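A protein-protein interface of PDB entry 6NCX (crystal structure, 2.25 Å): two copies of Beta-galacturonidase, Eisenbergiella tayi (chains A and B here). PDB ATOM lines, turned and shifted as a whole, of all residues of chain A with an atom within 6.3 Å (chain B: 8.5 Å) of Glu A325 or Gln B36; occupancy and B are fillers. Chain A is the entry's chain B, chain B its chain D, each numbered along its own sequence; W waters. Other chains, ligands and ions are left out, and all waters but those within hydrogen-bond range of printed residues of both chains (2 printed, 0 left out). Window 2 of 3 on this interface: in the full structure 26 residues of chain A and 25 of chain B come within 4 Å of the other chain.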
ATOM      1  N   THR A   4     -22.710  12.202   7.675  1.00  0.00           N
ATOM      2  CA  THR A   4     -23.023  11.370   6.515  1.00  0.00           C
ATOM      3  C   THR A   4     -24.514  11.381   6.184  1.00  0.00           C
ATOM      4  O   THR A   4     -24.939  10.678   5.256  1.00  0.00           O
ATOM      5  CB  THR A   4     -22.533   9.921   6.717  1.00  0.00           C
ATOM      6  OG1 THR A   4     -23.044   9.395   7.942  1.00  0.00           O
ATOM      7  CG2 THR A   4     -21.023   9.864   6.757  1.00  0.00           C
ATOM      8  N   PHE A   5     -25.299  12.184   6.904  1.00  0.00           N
ATOM      9  CA  PHE A   5     -26.744  12.232   6.767  1.00  0.00           C
ATOM     10  C   PHE A   5     -27.202  13.652   7.094  1.00  0.00           C
ATOM     11  O   PHE A   5     -26.520  14.398   7.805  1.00  0.00           O
ATOM     12  CB  PHE A   5     -27.426  11.191   7.680  1.00  0.00           C
ATOM     13  CG  PHE A   5     -27.227  11.458   9.143  1.00  0.00           C
ATOM     14  CD1 PHE A   5     -28.170  12.177   9.864  1.00  0.00           C
ATOM     15  CD2 PHE A   5     -26.078  11.018   9.792  1.00  0.00           C
ATOM     16  CE1 PHE A   5     -27.975  12.448  11.211  1.00  0.00           C
ATOM     17  CE2 PHE A   5     -25.874  11.283  11.128  1.00  0.00           C
ATOM     18  CZ  PHE A   5     -26.827  12.005  11.841  1.00  0.00           C
ATOM     19  N   TRP A 223     -28.053  -3.326  16.342  1.00  0.00           N
ATOM     20  CA  TRP A 223     -26.782  -2.862  15.801  1.00  0.00           C
ATOM     21  C   TRP A 223     -25.657  -3.711  16.387  1.00  0.00           C
ATOM     22  O   TRP A 223     -25.629  -3.954  17.600  1.00  0.00           O
ATOM     23  CB  TRP A 223     -26.574  -1.382  16.151  1.00  0.00           C
ATOM     24  CG  TRP A 223     -25.324  -0.721  15.583  1.00  0.00           C
ATOM     25  CD1 TRP A 223     -25.256   0.087  14.477  1.00  0.00           C
ATOM     26  CD2 TRP A 223     -23.988  -0.791  16.103  1.00  0.00           C
ATOM     27  NE1 TRP A 223     -23.971   0.509  14.273  1.00  0.00           N
ATOM     28  CE2 TRP A 223     -23.169  -0.013  15.255  1.00  0.00           C
ATOM     29  CE3 TRP A 223     -23.401  -1.443  17.196  1.00  0.00           C
ATOM     30  CZ2 TRP A 223     -21.795   0.133  15.469  1.00  0.00           C
ATOM     31  CZ3 TRP A 223     -22.042  -1.293  17.407  1.00  0.00           C
ATOM     32  CH2 TRP A 223     -21.253  -0.511  16.547  1.00  0.00           C
ATOM     33  N   PRO A 228     -24.447  -3.564  11.352  1.00  0.00           N
ATOM     34  CA  PRO A 228     -24.610  -2.203  11.927  1.00  0.00           C
ATOM     35  C   PRO A 228     -25.858  -1.496  11.400  1.00  0.00           C
ATOM     36  O   PRO A 228     -25.804  -0.512  10.634  1.00  0.00           O
ATOM     37  CB  PRO A 228     -23.303  -1.511  11.518  1.00  0.00           C
ATOM     38  CG  PRO A 228     -22.795  -2.270  10.296  1.00  0.00           C
ATOM     39  CD  PRO A 228     -23.594  -3.558  10.153  1.00  0.00           C
ATOM     40  N   LEU A 230     -28.829   0.939  11.421  1.00  0.00           N
ATOM     41  CA  LEU A 230     -29.065   2.272  11.957  1.00  0.00           C
ATOM     42  C   LEU A 230     -30.453   2.748  11.551  1.00  0.00           C
ATOM     43  O   LEU A 230     -30.936   2.418  10.465  1.00  0.00           O
ATOM     44  CB  LEU A 230     -28.018   3.265  11.443  1.00  0.00           C
ATOM     45  CG  LEU A 230     -26.559   3.044  11.816  1.00  0.00           C
ATOM     46  CD1 LEU A 230     -25.689   4.053  11.094  1.00  0.00           C
ATOM     47  CD2 LEU A 230     -26.399   3.177  13.325  1.00  0.00           C
ATOM     48  N   ARG A 250     -29.254   9.672  14.248  1.00  0.00           N
ATOM     49  CA  ARG A 250     -29.283   8.243  13.951  1.00  0.00           C
ATOM     50  C   ARG A 250     -28.968   7.451  15.205  1.00  0.00           C
ATOM     51  O   ARG A 250     -28.153   7.869  16.035  1.00  0.00           O
ATOM     52  CB  ARG A 250     -28.283   7.828  12.855  1.00  0.00           C
ATOM     53  CG  ARG A 250     -28.617   8.333  11.469  1.00  0.00           C
ATOM     54  CD  ARG A 250     -27.803   7.634  10.383  1.00  0.00           C
ATOM     55  NE  ARG A 250     -26.384   7.620  10.719  1.00  0.00           N
ATOM     56  CZ  ARG A 250     -25.408   7.347   9.864  1.00  0.00           C
ATOM     57  NH1 ARG A 250     -25.689   7.066   8.600  1.00  0.00           N
ATOM     58  NH2 ARG A 250     -24.150   7.353  10.275  1.00  0.00           N
ATOM     59  N   GLN A 294     -12.124   7.841   5.611  1.00  0.00           N
ATOM     60  CA  GLN A 294     -12.476   6.514   5.131  1.00  0.00           C
ATOM     61  C   GLN A 294     -11.242   5.720   4.709  1.00  0.00           C
ATOM     62  O   GLN A 294     -11.197   4.497   4.904  1.00  0.00           O
ATOM     63  CB  GLN A 294     -13.484   6.611   3.983  1.00  0.00           C
ATOM     64  CG  GLN A 294     -13.936   5.251   3.439  1.00  0.00           C
ATOM     65  CD  GLN A 294     -14.536   4.351   4.506  1.00  0.00           C
ATOM     66  OE1 GLN A 294     -14.921   4.816   5.576  1.00  0.00           O
ATOM     67  NE2 GLN A 294     -14.622   3.051   4.215  1.00  0.00           N
ATOM     68  N   MET A 298     -10.503   1.953   6.071  1.00  0.00           N
ATOM     69  CA  MET A 298     -10.304   0.760   5.248  1.00  0.00           C
ATOM     70  C   MET A 298      -8.996   0.051   5.598  1.00  0.00           C
ATOM     71  O   MET A 298      -8.937  -1.184   5.605  1.00  0.00           O
ATOM     72  CB  MET A 298     -10.354   1.126   3.761  1.00  0.00           C
ATOM     73  CG  MET A 298     -11.687   1.743   3.370  1.00  0.00           C
ATOM     74  SD  MET A 298     -11.941   2.052   1.614  1.00  0.00           S
ATOM     75  CE  MET A 298     -12.396   0.410   1.069  1.00  0.00           C
ATOM     76  N   LYS A 301      -9.713  -1.607   8.990  1.00  0.00           N
ATOM     77  CA  LYS A 301     -10.492  -2.823   8.796  1.00  0.00           C
ATOM     78  C   LYS A 301      -9.667  -3.906   8.113  1.00  0.00           C
ATOM     79  O   LYS A 301      -9.817  -5.090   8.425  1.00  0.00           O
ATOM     80  CB  LYS A 301     -11.769  -2.527   7.998  1.00  0.00           C
ATOM     81  CG  LYS A 301     -12.765  -1.682   8.789  1.00  0.00           C
ATOM     82  CD  LYS A 301     -14.129  -1.622   8.133  1.00  0.00           C
ATOM     83  CE  LYS A 301     -14.051  -1.156   6.694  1.00  0.00           C
ATOM     84  NZ  LYS A 301     -15.406  -1.251   6.062  1.00  0.00           N
ATOM     85  N   LEU A 320     -17.245   9.503  13.591  1.00  0.00           N
ATOM     86  CA  LEU A 320     -18.117   8.635  14.387  1.00  0.00           C
ATOM     87  C   LEU A 320     -19.292   8.113  13.560  1.00  0.00           C
ATOM     88  O   LEU A 320     -19.744   6.977  13.754  1.00  0.00           O
ATOM     89  CB  LEU A 320     -18.629   9.388  15.617  1.00  0.00           C
ATOM     90  CG  LEU A 320     -17.549   9.849  16.595  1.00  0.00           C
ATOM     91  CD1 LEU A 320     -18.159  10.677  17.749  1.00  0.00           C
ATOM     92  CD2 LEU A 320     -16.738   8.647  17.101  1.00  0.00           C
ATOM     93  N   ASP A 321     -19.834   8.955  12.674  1.00  0.00           N
ATOM     94  CA  ASP A 321     -20.838   8.495  11.721  1.00  0.00           C
ATOM     95  C   ASP A 321     -20.315   7.311  10.917  1.00  0.00           C
ATOM     96  O   ASP A 321     -21.017   6.309  10.738  1.00  0.00           O
ATOM     97  CB  ASP A 321     -21.239   9.628  10.770  1.00  0.00           C
ATOM     98  CG  ASP A 321     -22.202  10.619  11.396  1.00  0.00           C
ATOM     99  OD1 ASP A 321     -22.469  11.657  10.758  1.00  0.00           O
ATOM    100  OD2 ASP A 321     -22.675  10.376  12.530  1.00  0.00           O
ATOM    101  N   LEU A 322     -19.068   7.409  10.436  1.00  0.00           N
ATOM    102  CA  LEU A 322     -18.522   6.363   9.584  1.00  0.00           C
ATOM    103  C   LEU A 322     -18.322   5.068  10.360  1.00  0.00           C
ATOM    104  O   LEU A 322     -18.449   3.976   9.785  1.00  0.00           O
ATOM    105  CB  LEU A 322     -17.208   6.845   8.955  1.00  0.00           C
ATOM    106  CG  LEU A 322     -17.413   7.887   7.850  1.00  0.00           C
ATOM    107  CD1 LEU A 322     -16.088   8.506   7.460  1.00  0.00           C
ATOM    108  CD2 LEU A 322     -18.098   7.224   6.665  1.00  0.00           C
ATOM    109  N   CYS A 323     -18.032   5.185  11.663  1.00  0.00           N
ATOM    110  CA  CYS A 323     -17.860   4.023  12.526  1.00  0.00           C
ATOM    111  C   CYS A 323     -19.195   3.364  12.842  1.00  0.00           C
ATOM    112  O   CYS A 323     -19.291   2.133  12.863  1.00  0.00           O
ATOM    113  CB  CYS A 323     -17.167   4.432  13.824  1.00  0.00           C
ATOM    114  SG  CYS A 323     -15.466   4.891  13.676  1.00  0.00           S
ATOM    115  N   ASP A 324     -20.224   4.172  13.124  1.00  0.00           N
ATOM    116  CA  ASP A 324     -21.599   3.673  13.189  1.00  0.00           C
ATOM    117  C   ASP A 324     -21.956   2.825  11.962  1.00  0.00           C
ATOM    118  O   ASP A 324     -22.464   1.705  12.088  1.00  0.00           O
ATOM    119  CB  ASP A 324     -22.587   4.845  13.299  1.00  0.00           C
ATOM    120  CG  ASP A 324     -22.352   5.725  14.522  1.00  0.00           C
ATOM    121  OD1 ASP A 324     -21.666   5.308  15.476  1.00  0.00           O
ATOM    122  OD2 ASP A 324     -22.877   6.860  14.532  1.00  0.00           O
ATOM    123  N   GLU A 325     -21.723   3.366  10.762  1.00  0.00           N
ATOM    124  CA  GLU A 325     -22.149   2.703   9.528  1.00  0.00           C
ATOM    125  C   GLU A 325     -21.378   1.428   9.239  1.00  0.00           C
ATOM    126  O   GLU A 325     -21.866   0.588   8.480  1.00  0.00           O
ATOM    127  CB  GLU A 325     -21.990   3.632   8.324  1.00  0.00           C
ATOM    128  CG  GLU A 325     -22.753   4.902   8.459  1.00  0.00           C
ATOM    129  CD  GLU A 325     -22.725   5.745   7.205  1.00  0.00           C
ATOM    130  OE1 GLU A 325     -22.171   5.301   6.166  1.00  0.00           O
ATOM    131  OE2 GLU A 325     -23.276   6.859   7.261  1.00  0.00           O
ATOM    132  N   GLN A 326     -20.184   1.264   9.801  1.00  0.00           N
ATOM    133  CA  GLN A 326     -19.358   0.115   9.469  1.00  0.00           C
ATOM    134  C   GLN A 326     -19.176  -0.849  10.632  1.00  0.00           C
ATOM    135  O   GLN A 326     -18.419  -1.812  10.502  1.00  0.00           O
ATOM    136  CB  GLN A 326     -18.003   0.602   8.937  1.00  0.00           C
ATOM    137  CG  GLN A 326     -18.136   1.377   7.609  1.00  0.00           C
ATOM    138  CD  GLN A 326     -16.826   1.994   7.141  1.00  0.00           C
ATOM    139  OE1 GLN A 326     -16.077   1.384   6.382  1.00  0.00           O
ATOM    140  NE2 GLN A 326     -16.552   3.219   7.579  1.00  0.00           N
ATOM    141  N   GLY A 327     -19.852  -0.631  11.759  1.00  0.00           N
ATOM    142  CA  GLY A 327     -19.736  -1.553  12.876  1.00  0.00           C
ATOM    143  C   GLY A 327     -18.468  -1.441  13.690  1.00  0.00           C
ATOM    144  O   GLY A 327     -18.130  -2.382  14.411  1.00  0.00           O
ATOM    145  N   ILE A 328     -17.757  -0.319  13.609  1.00  0.00           N
ATOM    146  CA  ILE A 328     -16.525  -0.122  14.363  1.00  0.00           C
ATOM    147  C   ILE A 328     -16.876   0.366  15.761  1.00  0.00           C
ATOM    148  O   ILE A 328     -17.633   1.328  15.918  1.00  0.00           O
ATOM    149  CB  ILE A 328     -15.610   0.885  13.649  1.00  0.00           C
ATOM    150  CG1 ILE A 328     -15.465   0.521  12.167  1.00  0.00           C
ATOM    151  CG2 ILE A 328     -14.235   0.987  14.366  1.00  0.00           C
ATOM    152  CD1 ILE A 328     -14.531  -0.616  11.920  1.00  0.00           C
ATOM    153  N   SER B  18     -20.501  11.507  -1.493  1.00  0.00           N
ATOM    154  CA  SER B  18     -20.104  11.770  -0.103  1.00  0.00           C
ATOM    155  C   SER B  18     -20.735  10.743   0.838  1.00  0.00           C
ATOM    156  O   SER B  18     -21.338  11.076   1.864  1.00  0.00           O
ATOM    157  CB  SER B  18     -20.454  13.198   0.330  1.00  0.00           C
ATOM    158  OG  SER B  18     -19.706  14.156  -0.395  1.00  0.00           O
ATOM    159  N   ALA B  19     -20.595   9.472   0.474  1.00  0.00           N
ATOM    160  CA  ALA B  19     -21.251   8.400   1.208  1.00  0.00           C
ATOM    161  C   ALA B  19     -20.559   7.090   0.876  1.00  0.00           C
ATOM    162  O   ALA B  19     -19.812   6.988  -0.100  1.00  0.00           O
ATOM    163  CB  ALA B  19     -22.747   8.315   0.873  1.00  0.00           C
ATOM    164  N   LEU B  20     -20.824   6.090   1.705  1.00  0.00           N
ATOM    165  CA  LEU B  20     -20.393   4.728   1.438  1.00  0.00           C
ATOM    166  C   LEU B  20     -21.429   4.039   0.553  1.00  0.00           C
ATOM    167  O   LEU B  20     -22.629   4.094   0.836  1.00  0.00           O
ATOM    168  CB  LEU B  20     -20.220   3.957   2.746  1.00  0.00           C
ATOM    169  CG  LEU B  20     -19.275   4.539   3.793  1.00  0.00           C
ATOM    170  CD1 LEU B  20     -19.108   3.534   4.936  1.00  0.00           C
ATOM    171  CD2 LEU B  20     -17.921   4.909   3.170  1.00  0.00           C
ATOM    172  N   TRP B  21     -20.968   3.394  -0.513  1.00  0.00           N
ATOM    173  CA  TRP B  21     -21.823   2.506  -1.284  1.00  0.00           C
ATOM    174  C   TRP B  21     -21.344   1.076  -1.090  1.00  0.00           C
ATOM    175  O   TRP B  21     -20.247   0.830  -0.587  1.00  0.00           O
ATOM    176  CB  TRP B  21     -21.826   2.852  -2.783  1.00  0.00           C
ATOM    177  CG  TRP B  21     -22.338   4.237  -3.163  1.00  0.00           C
ATOM    178  CD1 TRP B  21     -22.307   5.374  -2.401  1.00  0.00           C
ATOM    179  CD2 TRP B  21     -22.917   4.618  -4.426  1.00  0.00           C
ATOM    180  NE1 TRP B  21     -22.833   6.433  -3.109  1.00  0.00           N
ATOM    181  CE2 TRP B  21     -23.219   5.997  -4.350  1.00  0.00           C
ATOM    182  CE3 TRP B  21     -23.209   3.924  -5.612  1.00  0.00           C
ATOM    183  CZ2 TRP B  21     -23.805   6.698  -5.415  1.00  0.00           C
ATOM    184  CZ3 TRP B  21     -23.805   4.618  -6.672  1.00  0.00           C
ATOM    185  CH2 TRP B  21     -24.088   5.990  -6.565  1.00  0.00           C
ATOM    186  N   ASN B  22     -22.181   0.130  -1.481  1.00  0.00           N
ATOM    187  CA  ASN B  22     -21.753  -1.259  -1.515  1.00  0.00           C
ATOM    188  C   ASN B  22     -20.954  -1.526  -2.786  1.00  0.00           C
ATOM    189  O   ASN B  22     -21.334  -1.089  -3.880  1.00  0.00           O
ATOM    190  CB  ASN B  22     -22.957  -2.192  -1.428  1.00  0.00           C
ATOM    191  CG  ASN B  22     -23.580  -2.188  -0.059  1.00  0.00           C
ATOM    192  OD1 ASN B  22     -22.895  -1.980   0.941  1.00  0.00           O
ATOM    193  ND2 ASN B  22     -24.883  -2.419   0.002  1.00  0.00           N
ATOM    194  N   PHE B  23     -19.844  -2.248  -2.634  1.00  0.00           N
ATOM    195  CA  PHE B  23     -18.867  -2.417  -3.697  1.00  0.00           C
ATOM    196  C   PHE B  23     -18.412  -3.867  -3.752  1.00  0.00           C
ATOM    197  O   PHE B  23     -18.175  -4.492  -2.715  1.00  0.00           O
ATOM    198  CB  PHE B  23     -17.654  -1.486  -3.475  1.00  0.00           C
ATOM    199  CG  PHE B  23     -16.495  -1.739  -4.412  1.00  0.00           C
ATOM    200  CD1 PHE B  23     -15.470  -2.602  -4.053  1.00  0.00           C
ATOM    201  CD2 PHE B  23     -16.428  -1.096  -5.645  1.00  0.00           C
ATOM    202  CE1 PHE B  23     -14.408  -2.830  -4.904  1.00  0.00           C
ATOM    203  CE2 PHE B  23     -15.370  -1.315  -6.504  1.00  0.00           C
ATOM    204  CZ  PHE B  23     -14.360  -2.187  -6.135  1.00  0.00           C
ATOM    205  N   HIS B  24     -18.285  -4.392  -4.968  1.00  0.00           N
ATOM    206  CA  HIS B  24     -17.650  -5.685  -5.176  1.00  0.00           C
ATOM    207  C   HIS B  24     -17.192  -5.758  -6.627  1.00  0.00           C
ATOM    208  O   HIS B  24     -17.813  -5.163  -7.513  1.00  0.00           O
ATOM    209  CB  HIS B  24     -18.590  -6.857  -4.831  1.00  0.00           C
ATOM    210  CG  HIS B  24     -19.873  -6.867  -5.606  1.00  0.00           C
ATOM    211  ND1 HIS B  24     -20.020  -7.545  -6.799  1.00  0.00           N
ATOM    212  CD2 HIS B  24     -21.072  -6.281  -5.357  1.00  0.00           C
ATOM    213  CE1 HIS B  24     -21.252  -7.379  -7.249  1.00  0.00           C
ATOM    214  NE2 HIS B  24     -21.910  -6.612  -6.394  1.00  0.00           N
ATOM    215  N   ALA B  33     -16.609 -10.692  -1.925  1.00  0.00           N
ATOM    216  CA  ALA B  33     -17.020  -9.987  -0.725  1.00  0.00           C
ATOM    217  C   ALA B  33     -17.594  -8.621  -1.081  1.00  0.00           C
ATOM    218  O   ALA B  33     -17.107  -7.937  -1.985  1.00  0.00           O
ATOM    219  CB  ALA B  33     -15.825  -9.833   0.221  1.00  0.00           C
ATOM    220  N   VAL B  34     -18.650  -8.235  -0.382  1.00  0.00           N
ATOM    221  CA  VAL B  34     -19.191  -6.889  -0.480  1.00  0.00           C
ATOM    222  C   VAL B  34     -18.537  -6.040   0.603  1.00  0.00           C
ATOM    223  O   VAL B  34     -18.603  -6.375   1.791  1.00  0.00           O
ATOM    224  CB  VAL B  34     -20.719  -6.893  -0.333  1.00  0.00           C
ATOM    225  CG1 VAL B  34     -21.281  -5.492  -0.551  1.00  0.00           C
ATOM    226  CG2 VAL B  34     -21.331  -7.883  -1.311  1.00  0.00           C
ATOM    227  N   ILE B  35     -17.895  -4.945   0.197  1.00  0.00           N
ATOM    228  CA  ILE B  35     -17.307  -4.009   1.143  1.00  0.00           C
ATOM    229  C   ILE B  35     -18.002  -2.660   1.007  1.00  0.00           C
ATOM    230  O   ILE B  35     -18.656  -2.357   0.005  1.00  0.00           O
ATOM    231  CB  ILE B  35     -15.781  -3.853   0.954  1.00  0.00           C
ATOM    232  CG1 ILE B  35     -15.477  -3.182  -0.383  1.00  0.00           C
ATOM    233  CG2 ILE B  35     -15.086  -5.209   1.047  1.00  0.00           C
ATOM    234  CD1 ILE B  35     -14.323  -2.205  -0.312  1.00  0.00           C
ATOM    235  N   GLN B  36     -17.846  -1.840   2.036  1.00  0.00           N
ATOM    236  CA  GLN B  36     -18.368  -0.480   2.029  1.00  0.00           C
ATOM    237  C   GLN B  36     -17.265   0.465   1.550  1.00  0.00           C
ATOM    238  O   GLN B  36     -16.251   0.652   2.233  1.00  0.00           O
ATOM    239  CB  GLN B  36     -18.895  -0.112   3.411  1.00  0.00           C
ATOM    240  CG  GLN B  36     -20.049  -1.021   3.838  1.00  0.00           C
ATOM    241  CD  GLN B  36     -20.419  -0.827   5.276  1.00  0.00           C
ATOM    242  OE1 GLN B  36     -19.716  -1.294   6.179  1.00  0.00           O
ATOM    243  NE2 GLN B  36     -21.521  -0.115   5.511  1.00  0.00           N
ATOM    244  N   ALA B  37     -17.462   1.042   0.363  1.00  0.00           N
ATOM    245  CA  ALA B  37     -16.472   1.837  -0.327  1.00  0.00           C
ATOM    246  C   ALA B  37     -16.915   3.289  -0.433  1.00  0.00           C
ATOM    247  O   ALA B  37     -18.098   3.563  -0.667  1.00  0.00           O
ATOM    248  CB  ALA B  37     -16.218   1.295  -1.733  1.00  0.00           C
ATOM    249  N   PRO B  38     -15.988   4.234  -0.297  1.00  0.00           N
ATOM    250  CA  PRO B  38     -16.354   5.648  -0.430  1.00  0.00           C
ATOM    251  C   PRO B  38     -16.656   6.020  -1.877  1.00  0.00           C
ATOM    252  O   PRO B  38     -15.997   5.566  -2.817  1.00  0.00           O
ATOM    253  CB  PRO B  38     -15.109   6.378   0.082  1.00  0.00           C
ATOM    254  CG  PRO B  38     -13.985   5.451  -0.292  1.00  0.00           C
ATOM    255  CD  PRO B  38     -14.542   4.062  -0.059  1.00  0.00           C
ATOM    256  N   VAL B  39     -17.680   6.845  -2.043  1.00  0.00           N
ATOM    257  CA  VAL B  39     -17.965   7.533  -3.292  1.00  0.00           C
ATOM    258  C   VAL B  39     -17.998   9.015  -2.940  1.00  0.00           C
ATOM    259  O   VAL B  39     -18.746   9.411  -2.043  1.00  0.00           O
ATOM    260  CB  VAL B  39     -19.298   7.081  -3.915  1.00  0.00           C
ATOM    261  CG1 VAL B  39     -19.605   7.853  -5.211  1.00  0.00           C
ATOM    262  CG2 VAL B  39     -19.323   5.565  -4.130  1.00  0.00           C
ATOM    263  N   TYR B  46      -8.614   1.018  -2.460  1.00  0.00           N
ATOM    264  CA  TYR B  46      -9.155   0.104  -1.457  1.00  0.00           C
ATOM    265  C   TYR B  46      -8.203  -1.073  -1.299  1.00  0.00           C
ATOM    266  O   TYR B  46      -7.794  -1.657  -2.308  1.00  0.00           O
ATOM    267  CB  TYR B  46     -10.536  -0.418  -1.845  1.00  0.00           C
ATOM    268  CG  TYR B  46     -11.510   0.596  -2.433  1.00  0.00           C
ATOM    269  CD1 TYR B  46     -12.589   0.169  -3.202  1.00  0.00           C
ATOM    270  CD2 TYR B  46     -11.369   1.964  -2.208  1.00  0.00           C
ATOM    271  CE1 TYR B  46     -13.478   1.065  -3.756  1.00  0.00           C
ATOM    272  CE2 TYR B  46     -12.260   2.876  -2.755  1.00  0.00           C
ATOM    273  CZ  TYR B  46     -13.316   2.418  -3.529  1.00  0.00           C
ATOM    274  OH  TYR B  46     -14.214   3.312  -4.077  1.00  0.00           O
ATOM    275  N   PRO B  47      -7.839  -1.449  -0.055  1.00  0.00           N
ATOM    276  CA  PRO B  47      -6.835  -2.510   0.157  1.00  0.00           C
ATOM    277  C   PRO B  47      -6.964  -3.749  -0.728  1.00  0.00           C
ATOM    278  O   PRO B  47      -5.941  -4.245  -1.207  1.00  0.00           O
ATOM    279  CB  PRO B  47      -7.029  -2.873   1.637  1.00  0.00           C
ATOM    280  CG  PRO B  47      -7.513  -1.602   2.270  1.00  0.00           C
ATOM    281  CD  PRO B  47      -8.379  -0.927   1.214  1.00  0.00           C
ATOM    282  N   TYR B  58     -20.928  -0.751  -7.953  1.00  0.00           N
ATOM    283  CA  TYR B  58     -21.272   0.142  -6.851  1.00  0.00           C
ATOM    284  C   TYR B  58     -22.788   0.232  -6.753  1.00  0.00           C
ATOM    285  O   TYR B  58     -23.467   0.337  -7.778  1.00  0.00           O
ATOM    286  CB  TYR B  58     -20.712   1.558  -7.072  1.00  0.00           C
ATOM    287  CG  TYR B  58     -19.207   1.709  -6.986  1.00  0.00           C
ATOM    288  CD1 TYR B  58     -18.605   2.246  -5.846  1.00  0.00           C
ATOM    289  CD2 TYR B  58     -18.389   1.338  -8.048  1.00  0.00           C
ATOM    290  CE1 TYR B  58     -17.230   2.397  -5.761  1.00  0.00           C
ATOM    291  CE2 TYR B  58     -17.013   1.486  -7.972  1.00  0.00           C
ATOM    292  CZ  TYR B  58     -16.433   2.016  -6.833  1.00  0.00           C
ATOM    293  OH  TYR B  58     -15.052   2.160  -6.765  1.00  0.00           O
ATOM    294  N   SER B  59     -23.332   0.219  -5.536  1.00  0.00           N
ATOM    295  CA  SER B  59     -24.789   0.266  -5.396  1.00  0.00           C
ATOM    296  C   SER B  59     -25.203   0.897  -4.073  1.00  0.00           C
ATOM    297  O   SER B  59     -24.504   0.789  -3.062  1.00  0.00           O
ATOM    298  CB  SER B  59     -25.432  -1.128  -5.520  1.00  0.00           C
ATOM    299  OG  SER B  59     -24.800  -2.074  -4.675  1.00  0.00           O
HETATM  300  O   HOH W   1     -17.117  -2.866   4.683  1.00  0.00           O
HETATM  301  O   HOH W   2     -22.214   6.868   4.185  1.00  0.00           O
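Gln A294 touches Leu B20 (CD to CD2, 3.7 Å).
NE2 of Gln A294 touches O of Gln B36 (3.5 Å).
Pro B38 touches Gln A294 (CB to CG, 3.7 Å).
CE of Met A298 touches CD1 of Ile B35, at 3.5 Å.
Met A298 touches Pro B38.
Tyr B46 touches Met A298.
Met A298 touches Pro B47 (O to CG, 3.7 Å).
Glu A325 touches Leu B20.
Leu B20 touches Gln A326 (CD1 to CD, 3.5 Å).
Gln A326 touches Gln B36 (CG to OE1, 3.4 Å).
No position is printed for both chains.
NE2 of Gln B36 lies within hydrogen-bond range of O of Glu A325.
Of the 18 printed residues of chain A, 4 touch a printed residue of chain B.
Printed residues of chain B that touch a printed residue of chain A: Leu B20, Ile B35, Gln B36, Pro B38, Tyr B46 and Pro B47.
Hydrophobic or aromatic side chains of chain B within 4 Å of the printed part of chain A: Leu B20, Ile B35, Pro B38, Tyr B46 and Pro B47.
Among the printed residues, 11 pairs touch across the chains.
Among the printed residues, no Asp or Glu carboxylate lies within 4 Å of a Lys or Arg side-chain nitrogen of the other chain.
Printed residues of chain B within 4 Å of Gln A294: Leu B20 (3.7 Å), Gln B36 (3.5 Å) and Pro B38 (3.7 Å).
Printed residues of chain B within 4 Å of Met A298: Ile B35 (3.5 Å), Pro B38 (3.7 Å), Tyr B46 (3.6 Å) and Pro B47 (3.7 Å).
Of chain B, only Leu B20 (3.7 Å) and Gln B36 (3.1 Å) come within 4 Å of Glu A325.
Ala B19 touches none of the printed residues of chain A.
Asn B22 touches none of the printed residues of chain A.
Of the printed residues of chain A, Pro B38 touches Gln A294 and Met A298.
Printed residues of chain A within 4 Å of Tyr B46: Met A298 (3.6 Å).
The nearest residue of chain A that does not touch Gln B36 is Met A298 (4.03 Å).
The side-chain amide oxygen of Gln A294 lies within hydrogen-bond range of the side-chain amide nitrogen of Gln A326.
O of Pro B38 is in hydrogen-bond range of OH of Tyr B46 (3.1 Å).
The backbone NH (N) of Phe B23 sits at hydrogen-bond distance from the backbone carbonyl oxygen (O) of Ile B35 (2.9 Å).
The side-chain hydroxyl of Tyr B46 is in hydrogen-bond range of the side-chain hydroxyl of Tyr B58, 3.0 Å away.
The side-chain hydroxyl of Thr A4 is in hydrogen-bond range of the side-chain carboxylate of Glu A325 (2.6 Å).
The side-chain amide oxygen of Gln A326 lies within hydrogen-bond range of the side-chain amino group of Lys A301 (2.7 Å).
Water W2 lies within hydrogen-bond range of OE1 of Glu A325 and N of Leu B20.
Water W1 lies within hydrogen-bond range of NZ of Lys A301 and N of Gln B36.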
